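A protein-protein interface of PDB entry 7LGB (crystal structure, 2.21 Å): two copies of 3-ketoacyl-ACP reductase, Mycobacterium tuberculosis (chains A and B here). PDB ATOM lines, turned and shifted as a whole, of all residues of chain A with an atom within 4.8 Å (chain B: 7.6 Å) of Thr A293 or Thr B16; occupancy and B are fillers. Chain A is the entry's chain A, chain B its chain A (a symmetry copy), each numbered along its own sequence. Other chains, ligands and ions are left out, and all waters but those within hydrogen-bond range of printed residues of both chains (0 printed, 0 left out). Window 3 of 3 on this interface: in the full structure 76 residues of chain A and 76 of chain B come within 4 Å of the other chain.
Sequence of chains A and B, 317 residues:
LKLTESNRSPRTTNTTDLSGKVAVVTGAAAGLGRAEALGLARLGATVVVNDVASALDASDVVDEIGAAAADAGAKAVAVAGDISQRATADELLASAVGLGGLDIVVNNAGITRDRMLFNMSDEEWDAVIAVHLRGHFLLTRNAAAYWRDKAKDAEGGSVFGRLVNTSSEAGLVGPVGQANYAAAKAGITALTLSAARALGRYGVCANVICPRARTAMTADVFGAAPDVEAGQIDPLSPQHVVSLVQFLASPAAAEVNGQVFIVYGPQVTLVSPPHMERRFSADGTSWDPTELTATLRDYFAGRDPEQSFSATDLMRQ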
ATOM      1  N   PRO A 289     -10.893   0.713 -14.227  1.00  0.00           N
ATOM      2  CA  PRO A 289     -12.310   0.911 -14.582  1.00  0.00           C
ATOM      3  C   PRO A 289     -12.626   0.609 -16.041  1.00  0.00           C
ATOM      4  O   PRO A 289     -13.656  -0.009 -16.319  1.00  0.00           O
ATOM      5  CB  PRO A 289     -12.558   2.385 -14.228  1.00  0.00           C
ATOM      6  CG  PRO A 289     -11.462   2.741 -13.256  1.00  0.00           C
ATOM      7  CD  PRO A 289     -10.278   1.929 -13.668  1.00  0.00           C
ATOM      8  N   THR A 290     -11.773   1.000 -16.986  1.00  0.00           N
ATOM      9  CA  THR A 290     -12.081   0.660 -18.370  1.00  0.00           C
ATOM     10  C   THR A 290     -11.981  -0.844 -18.595  1.00  0.00           C
ATOM     11  O   THR A 290     -12.703  -1.397 -19.432  1.00  0.00           O
ATOM     12  CB  THR A 290     -11.171   1.430 -19.342  1.00  0.00           C
ATOM     13  OG1 THR A 290      -9.869   0.845 -19.362  1.00  0.00           O
ATOM     14  CG2 THR A 290     -11.047   2.890 -18.929  1.00  0.00           C
ATOM     15  N   GLU A 291     -11.121  -1.523 -17.833  1.00  0.00           N
ATOM     16  CA  GLU A 291     -11.020  -2.975 -17.930  1.00  0.00           C
ATOM     17  C   GLU A 291     -12.246  -3.659 -17.338  1.00  0.00           C
ATOM     18  O   GLU A 291     -12.757  -4.632 -17.906  1.00  0.00           O
ATOM     19  CB  GLU A 291      -9.757  -3.456 -17.224  1.00  0.00           C
ATOM     20  CG  GLU A 291      -9.308  -4.822 -17.657  1.00  0.00           C
ATOM     21  CD  GLU A 291      -8.478  -4.760 -18.911  1.00  0.00           C
ATOM     22  OE1 GLU A 291      -7.718  -3.779 -19.063  1.00  0.00           O
ATOM     23  OE2 GLU A 291      -8.590  -5.681 -19.748  1.00  0.00           O
ATOM     24  N   LEU A 292     -12.717  -3.185 -16.183  1.00  0.00           N
ATOM     25  CA  LEU A 292     -13.952  -3.725 -15.631  1.00  0.00           C
ATOM     26  C   LEU A 292     -15.097  -3.560 -16.620  1.00  0.00           C
ATOM     27  O   LEU A 292     -15.879  -4.492 -16.847  1.00  0.00           O
ATOM     28  CB  LEU A 292     -14.277  -3.037 -14.307  1.00  0.00           C
ATOM     29  CG  LEU A 292     -15.635  -3.376 -13.703  1.00  0.00           C
ATOM     30  CD1 LEU A 292     -15.705  -4.868 -13.377  1.00  0.00           C
ATOM     31  CD2 LEU A 292     -15.912  -2.510 -12.448  1.00  0.00           C
ATOM     32  N   THR A 293     -15.194  -2.376 -17.228  1.00  0.00           N
ATOM     33  CA  THR A 293     -16.218  -2.117 -18.231  1.00  0.00           C
ATOM     34  C   THR A 293     -16.133  -3.129 -19.359  1.00  0.00           C
ATOM     35  O   THR A 293     -17.144  -3.721 -19.755  1.00  0.00           O
ATOM     36  CB  THR A 293     -16.059  -0.693 -18.770  1.00  0.00           C
ATOM     37  OG1 THR A 293     -16.500   0.241 -17.772  1.00  0.00           O
ATOM     38  CG2 THR A 293     -16.862  -0.500 -20.052  1.00  0.00           C
ATOM     39  N   ALA A 294     -14.922  -3.369 -19.863  1.00  0.00           N
ATOM     40  CA  ALA A 294     -14.747  -4.326 -20.948  1.00  0.00           C
ATOM     41  C   ALA A 294     -15.185  -5.723 -20.529  1.00  0.00           C
ATOM     42  O   ALA A 294     -15.836  -6.431 -21.301  1.00  0.00           O
ATOM     43  CB  ALA A 294     -13.291  -4.328 -21.416  1.00  0.00           C
ATOM     44  N   THR A 295     -14.869  -6.121 -19.295  1.00  0.00           N
ATOM     45  CA  THR A 295     -15.182  -7.473 -18.843  1.00  0.00           C
ATOM     46  C   THR A 295     -16.685  -7.674 -18.710  1.00  0.00           C
ATOM     47  O   THR A 295     -17.230  -8.683 -19.175  1.00  0.00           O
ATOM     48  CB  THR A 295     -14.485  -7.745 -17.509  1.00  0.00           C
ATOM     49  OG1 THR A 295     -13.070  -7.590 -17.674  1.00  0.00           O
ATOM     50  CG2 THR A 295     -14.797  -9.162 -17.000  1.00  0.00           C
ATOM     51  N   LEU A 296     -17.369  -6.721 -18.067  1.00  0.00           N
ATOM     52  CA  LEU A 296     -18.810  -6.831 -17.868  1.00  0.00           C
ATOM     53  C   LEU A 296     -19.560  -6.717 -19.190  1.00  0.00           C
ATOM     54  O   LEU A 296     -20.518  -7.457 -19.428  1.00  0.00           O
ATOM     55  CB  LEU A 296     -19.282  -5.767 -16.886  1.00  0.00           C
ATOM     56  CG  LEU A 296     -18.720  -5.944 -15.466  1.00  0.00           C
ATOM     57  CD1 LEU A 296     -19.226  -4.868 -14.520  1.00  0.00           C
ATOM     58  CD2 LEU A 296     -19.055  -7.327 -14.920  1.00  0.00           C
ATOM     59  N   ARG A 297     -19.130  -5.802 -20.059  1.00  0.00           N
ATOM     60  CA  ARG A 297     -19.802  -5.613 -21.339  1.00  0.00           C
ATOM     61  C   ARG A 297     -19.722  -6.879 -22.181  1.00  0.00           C
ATOM     62  O   ARG A 297     -20.699  -7.272 -22.828  1.00  0.00           O
ATOM     63  CB  ARG A 297     -19.171  -4.423 -22.069  1.00  0.00           C
ATOM     64  CG  ARG A 297     -19.850  -3.997 -23.356  1.00  0.00           C
ATOM     65  CD  ARG A 297     -19.194  -2.746 -23.923  1.00  0.00           C
ATOM     66  NE  ARG A 297     -20.070  -2.035 -24.851  1.00  0.00           N
ATOM     67  N   ASP A 298     -18.569  -7.543 -22.162  1.00  0.00           N
ATOM     68  CA  ASP A 298     -18.424  -8.794 -22.890  1.00  0.00           C
ATOM     69  C   ASP A 298     -19.284  -9.893 -22.279  1.00  0.00           C
ATOM     70  O   ASP A 298     -19.886 -10.692 -23.006  1.00  0.00           O
ATOM     71  CB  ASP A 298     -16.955  -9.214 -22.917  1.00  0.00           C
ATOM     72  CG  ASP A 298     -16.772 -10.648 -23.371  1.00  0.00           C
ATOM     73  OD1 ASP A 298     -16.681 -10.877 -24.596  1.00  0.00           O
ATOM     74  OD2 ASP A 298     -16.727 -11.547 -22.504  1.00  0.00           O
ATOM     75  N   THR B  16     -15.995   5.306 -21.441  1.00  0.00           N
ATOM     76  CA  THR B  16     -17.181   5.457 -20.604  1.00  0.00           C
ATOM     77  C   THR B  16     -17.411   6.917 -20.212  1.00  0.00           C
ATOM     78  O   THR B  16     -17.732   7.209 -19.059  1.00  0.00           O
ATOM     79  CB  THR B  16     -17.074   4.615 -19.320  1.00  0.00           C
ATOM     80  OG1 THR B  16     -15.851   4.926 -18.643  1.00  0.00           O
ATOM     81  CG2 THR B  16     -17.100   3.134 -19.648  1.00  0.00           C
ATOM     82  N   ASP B  17     -17.264   7.823 -21.181  1.00  0.00           N
ATOM     83  CA  ASP B  17     -17.307   9.255 -20.912  1.00  0.00           C
ATOM     84  C   ASP B  17     -18.741   9.745 -20.719  1.00  0.00           C
ATOM     85  O   ASP B  17     -19.624   9.451 -21.528  1.00  0.00           O
ATOM     86  CB  ASP B  17     -16.640  10.018 -22.050  1.00  0.00           C
ATOM     87  CG  ASP B  17     -16.697  11.511 -21.852  1.00  0.00           C
ATOM     88  OD1 ASP B  17     -16.002  12.026 -20.947  1.00  0.00           O
ATOM     89  OD2 ASP B  17     -17.444  12.165 -22.602  1.00  0.00           O
ATOM     90  N   LEU B  18     -18.968  10.507 -19.650  1.00  0.00           N
ATOM     91  CA  LEU B  18     -20.302  10.968 -19.279  1.00  0.00           C
ATOM     92  C   LEU B  18     -20.504  12.456 -19.551  1.00  0.00           C
ATOM     93  O   LEU B  18     -21.399  13.073 -18.963  1.00  0.00           O
ATOM     94  CB  LEU B  18     -20.582  10.666 -17.805  1.00  0.00           C
ATOM     95  CG  LEU B  18     -20.507   9.208 -17.365  1.00  0.00           C
ATOM     96  CD1 LEU B  18     -20.921   9.096 -15.908  1.00  0.00           C
ATOM     97  CD2 LEU B  18     -21.382   8.324 -18.272  1.00  0.00           C
ATOM     98  N   SER B  19     -19.671  13.044 -20.411  1.00  0.00           N
ATOM     99  CA  SER B  19     -19.831  14.433 -20.822  1.00  0.00           C
ATOM    100  C   SER B  19     -21.255  14.707 -21.284  1.00  0.00           C
ATOM    101  O   SER B  19     -21.866  13.885 -21.972  1.00  0.00           O
ATOM    102  CB  SER B  19     -18.857  14.753 -21.962  1.00  0.00           C
ATOM    103  OG  SER B  19     -17.518  14.711 -21.515  1.00  0.00           O
ATOM    104  N   GLY B  39     -16.707  10.348  -8.697  1.00  0.00           N
ATOM    105  CA  GLY B  39     -16.350   9.493  -9.816  1.00  0.00           C
ATOM    106  C   GLY B  39     -17.147   9.807 -11.071  1.00  0.00           C
ATOM    107  O   GLY B  39     -16.641   9.677 -12.188  1.00  0.00           O
ATOM    108  N   LEU B  40     -18.408  10.198 -10.908  1.00  0.00           N
ATOM    109  CA  LEU B  40     -19.192  10.599 -12.066  1.00  0.00           C
ATOM    110  C   LEU B  40     -18.706  11.942 -12.594  1.00  0.00           C
ATOM    111  O   LEU B  40     -18.557  12.116 -13.806  1.00  0.00           O
ATOM    112  CB  LEU B  40     -20.674  10.654 -11.706  1.00  0.00           C
ATOM    113  CG  LEU B  40     -21.327   9.345 -11.245  1.00  0.00           C
ATOM    114  CD1 LEU B  40     -22.820   9.554 -10.932  1.00  0.00           C
ATOM    115  CD2 LEU B  40     -21.144   8.255 -12.294  1.00  0.00           C
ATOM    116  N   ARG B  42     -15.709  13.094 -12.461  1.00  0.00           N
ATOM    117  CA  ARG B  42     -14.439  12.893 -13.158  1.00  0.00           C
ATOM    118  C   ARG B  42     -14.630  12.379 -14.581  1.00  0.00           C
ATOM    119  O   ARG B  42     -13.740  12.551 -15.412  1.00  0.00           O
ATOM    120  CB  ARG B  42     -13.544  11.922 -12.377  1.00  0.00           C
ATOM    121  CG  ARG B  42     -12.916  12.518 -11.118  1.00  0.00           C
ATOM    122  CD  ARG B  42     -11.803  11.626 -10.554  1.00  0.00           C
ATOM    123  NE  ARG B  42     -12.188  10.214 -10.453  1.00  0.00           N
ATOM    124  CZ  ARG B  42     -12.661   9.633  -9.349  1.00  0.00           C
ATOM    125  NH1 ARG B  42     -12.816  10.340  -8.236  1.00  0.00           N
ATOM    126  NH2 ARG B  42     -12.976   8.341  -9.353  1.00  0.00           N
ATOM    127  N   LEU B  43     -15.753  11.739 -14.871  1.00  0.00           N
ATOM    128  CA  LEU B  43     -16.072  11.283 -16.213  1.00  0.00           C
ATOM    129  C   LEU B  43     -16.778  12.344 -17.042  1.00  0.00           C
ATOM    130  O   LEU B  43     -17.121  12.072 -18.196  1.00  0.00           O
ATOM    131  CB  LEU B  43     -16.938  10.022 -16.141  1.00  0.00           C
ATOM    132  CG  LEU B  43     -16.237   8.841 -15.464  1.00  0.00           C
ATOM    133  CD1 LEU B  43     -17.176   7.646 -15.301  1.00  0.00           C
ATOM    134  CD2 LEU B  43     -14.971   8.460 -16.216  1.00  0.00           C
ATOM    135  N   GLY B  44     -16.995  13.541 -16.488  1.00  0.00           N
ATOM    136  CA  GLY B  44     -17.620  14.631 -17.217  1.00  0.00           C
ATOM    137  C   GLY B  44     -19.069  14.898 -16.859  1.00  0.00           C
ATOM    138  O   GLY B  44     -19.679  15.806 -17.434  1.00  0.00           O
ATOM    139  N   SER B 243     -15.909   2.306  -9.187  1.00  0.00           N
ATOM    140  CA  SER B 243     -15.612   1.764 -10.512  1.00  0.00           C
ATOM    141  C   SER B 243     -16.826   1.055 -11.107  1.00  0.00           C
ATOM    142  O   SER B 243     -17.137   1.235 -12.291  1.00  0.00           O
ATOM    143  CB  SER B 243     -14.422   0.812 -10.443  1.00  0.00           C
ATOM    144  OG  SER B 243     -13.245   1.496 -10.079  1.00  0.00           O
ATOM    145  N   LEU B 244     -17.538   0.265 -10.298  1.00  0.00           N
ATOM    146  CA  LEU B 244     -18.747  -0.375 -10.807  1.00  0.00           C
ATOM    147  C   LEU B 244     -19.837   0.648 -11.091  1.00  0.00           C
ATOM    148  O   LEU B 244     -20.517   0.566 -12.123  1.00  0.00           O
ATOM    149  CB  LEU B 244     -19.259  -1.424  -9.824  1.00  0.00           C
ATOM    150  CG  LEU B 244     -20.522  -2.169 -10.258  1.00  0.00           C
ATOM    151  CD1 LEU B 244     -20.299  -2.863 -11.612  1.00  0.00           C
ATOM    152  CD2 LEU B 244     -20.954  -3.169  -9.198  1.00  0.00           C
ATOM    153  N   GLN B 246     -19.612   3.762 -11.938  1.00  0.00           N
ATOM    154  CA  GLN B 246     -19.288   4.470 -13.175  1.00  0.00           C
ATOM    155  C   GLN B 246     -19.740   3.680 -14.397  1.00  0.00           C
ATOM    156  O   GLN B 246     -20.292   4.249 -15.344  1.00  0.00           O
ATOM    157  CB  GLN B 246     -17.782   4.737 -13.255  1.00  0.00           C
ATOM    158  CG  GLN B 246     -17.277   5.751 -12.241  1.00  0.00           C
ATOM    159  CD  GLN B 246     -15.765   5.873 -12.247  1.00  0.00           C
ATOM    160  OE1 GLN B 246     -15.052   4.872 -12.311  1.00  0.00           O
ATOM    161  NE2 GLN B 246     -15.271   7.102 -12.189  1.00  0.00           N
ATOM    162  N   PHE B 247     -19.488   2.369 -14.399  1.00  0.00           N
ATOM    163  CA  PHE B 247     -19.940   1.524 -15.499  1.00  0.00           C
ATOM    164  C   PHE B 247     -21.458   1.517 -15.597  1.00  0.00           C
ATOM    165  O   PHE B 247     -22.030   1.758 -16.669  1.00  0.00           O
ATOM    166  CB  PHE B 247     -19.421   0.096 -15.317  1.00  0.00           C
ATOM    167  CG  PHE B 247     -20.085  -0.898 -16.224  1.00  0.00           C
ATOM    168  CD1 PHE B 247     -19.817  -0.896 -17.582  1.00  0.00           C
ATOM    169  CD2 PHE B 247     -20.999  -1.813 -15.723  1.00  0.00           C
ATOM    170  CE1 PHE B 247     -20.436  -1.805 -18.426  1.00  0.00           C
ATOM    171  CE2 PHE B 247     -21.615  -2.719 -16.550  1.00  0.00           C
ATOM    172  CZ  PHE B 247     -21.337  -2.721 -17.908  1.00  0.00           C
ATOM    173  N   LEU B 248     -22.130   1.239 -14.478  1.00  0.00           N
ATOM    174  CA  LEU B 248     -23.579   1.099 -14.465  1.00  0.00           C
ATOM    175  C   LEU B 248     -24.289   2.397 -14.791  1.00  0.00           C
ATOM    176  O   LEU B 248     -25.495   2.373 -15.044  1.00  0.00           O
ATOM    177  CB  LEU B 248     -24.042   0.613 -13.099  1.00  0.00           C
ATOM    178  CG  LEU B 248     -23.621  -0.790 -12.671  1.00  0.00           C
ATOM    179  CD1 LEU B 248     -24.235  -1.086 -11.299  1.00  0.00           C
ATOM    180  CD2 LEU B 248     -24.059  -1.812 -13.714  1.00  0.00           C
ATOM    181  N   ALA B 249     -23.574   3.518 -14.757  1.00  0.00           N
ATOM    182  CA  ALA B 249     -24.129   4.819 -15.074  1.00  0.00           C
ATOM    183  C   ALA B 249     -23.882   5.213 -16.517  1.00  0.00           C
ATOM    184  O   ALA B 249     -24.276   6.314 -16.919  1.00  0.00           O
ATOM    185  CB  ALA B 249     -23.526   5.881 -14.158  1.00  0.00           C
ATOM    186  N   SER B 250     -23.239   4.349 -17.295  1.00  0.00           N
ATOM    187  CA  SER B 250     -22.644   4.739 -18.561  1.00  0.00           C
ATOM    188  C   SER B 250     -23.383   4.133 -19.750  1.00  0.00           C
ATOM    189  O   SER B 250     -24.133   3.161 -19.607  1.00  0.00           O
ATOM    190  CB  SER B 250     -21.171   4.305 -18.607  1.00  0.00           C
ATOM    191  OG  SER B 250     -21.062   2.937 -18.948  1.00  0.00           O
ATOM    192  N   PRO B 251     -23.185   4.692 -20.949  1.00  0.00           N
ATOM    193  CA  PRO B 251     -23.647   4.010 -22.168  1.00  0.00           C
ATOM    194  C   PRO B 251     -23.216   2.560 -22.251  1.00  0.00           C
ATOM    195  O   PRO B 251     -23.973   1.734 -22.766  1.00  0.00           O
ATOM    196  CB  PRO B 251     -23.008   4.841 -23.291  1.00  0.00           C
ATOM    197  CG  PRO B 251     -22.876   6.193 -22.711  1.00  0.00           C
ATOM    198  CD  PRO B 251     -22.566   5.996 -21.250  1.00  0.00           C
ATOM    199  N   ALA B 252     -22.027   2.223 -21.746  1.00  0.00           N
ATOM    200  CA  ALA B 252     -21.492   0.879 -21.934  1.00  0.00           C
ATOM    201  C   ALA B 252     -22.315  -0.197 -21.228  1.00  0.00           C
ATOM    202  O   ALA B 252     -22.138  -1.384 -21.522  1.00  0.00           O
ATOM    203  CB  ALA B 252     -20.039   0.827 -21.456  1.00  0.00           C
ATOM    204  N   ALA B 253     -23.206   0.179 -20.305  1.00  0.00           N
ATOM    205  CA  ALA B 253     -24.034  -0.796 -19.602  1.00  0.00           C
ATOM    206  C   ALA B 253     -25.413  -0.986 -20.246  1.00  0.00           C
ATOM    207  O   ALA B 253     -26.351  -1.437 -19.571  1.00  0.00           O
ATOM    208  CB  ALA B 253     -24.183  -0.395 -18.135  1.00  0.00           C
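No position is printed for both chains.
Of the 9 pairs that touch across the chains among the printed residues, none has its exchanged pair printed and touching as well.
Of the printed residues of chain B, Pro A289 touches Ser B243 (3.8 Å).
Thr A293 touches just these residues of chain B: Thr B16, Phe B247 and Ala B252.
Printed residues of chain B within 4 Å of Arg A297: Ala B252 (3.9 Å).
Of the printed residues of chain A, Ser B243 touches Pro A289 and Leu A292.
Of the printed residues of chain A, Leu B244 touches Leu A292 and Leu A296.
The backbone carbonyl oxygen of Pro A289 lies within hydrogen-bond range of the side-chain hydroxyl of Thr A293.
The side-chain hydroxyl (OG) of Ser B250 sits at hydrogen-bond distance from the backbone carbonyl oxygen (O) of Phe B247 (2.7 Å).
OG of Ser B250 sits at hydrogen-bond distance from N of Ala B252 (3.0 Å).
Among the printed residues, merely in contact across the chains: Pro A289 with Ser B243 (3.8 Å), Leu A292 with Ser B243 (3.9 Å), Leu A292 with Leu B244 (3.9 Å), Thr A293 with Thr B16 (3.5 Å), Thr A293 with Phe B247 (3.5 Å), Thr A293 with Ala B252 (3.7 Å), Leu A296 with Leu B244 (3.7 Å), Leu A296 with Phe B247 (3.7 Å) and Arg A297 with Ala B252 (3.9 Å).
Of the 19 printed residues of chain B, 5 touch a printed residue of chain A.
Printed residues of chain A that touch a printed residue of chain B: Pro A289, Leu A292, Thr A293, Leu A296 and Arg A297.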
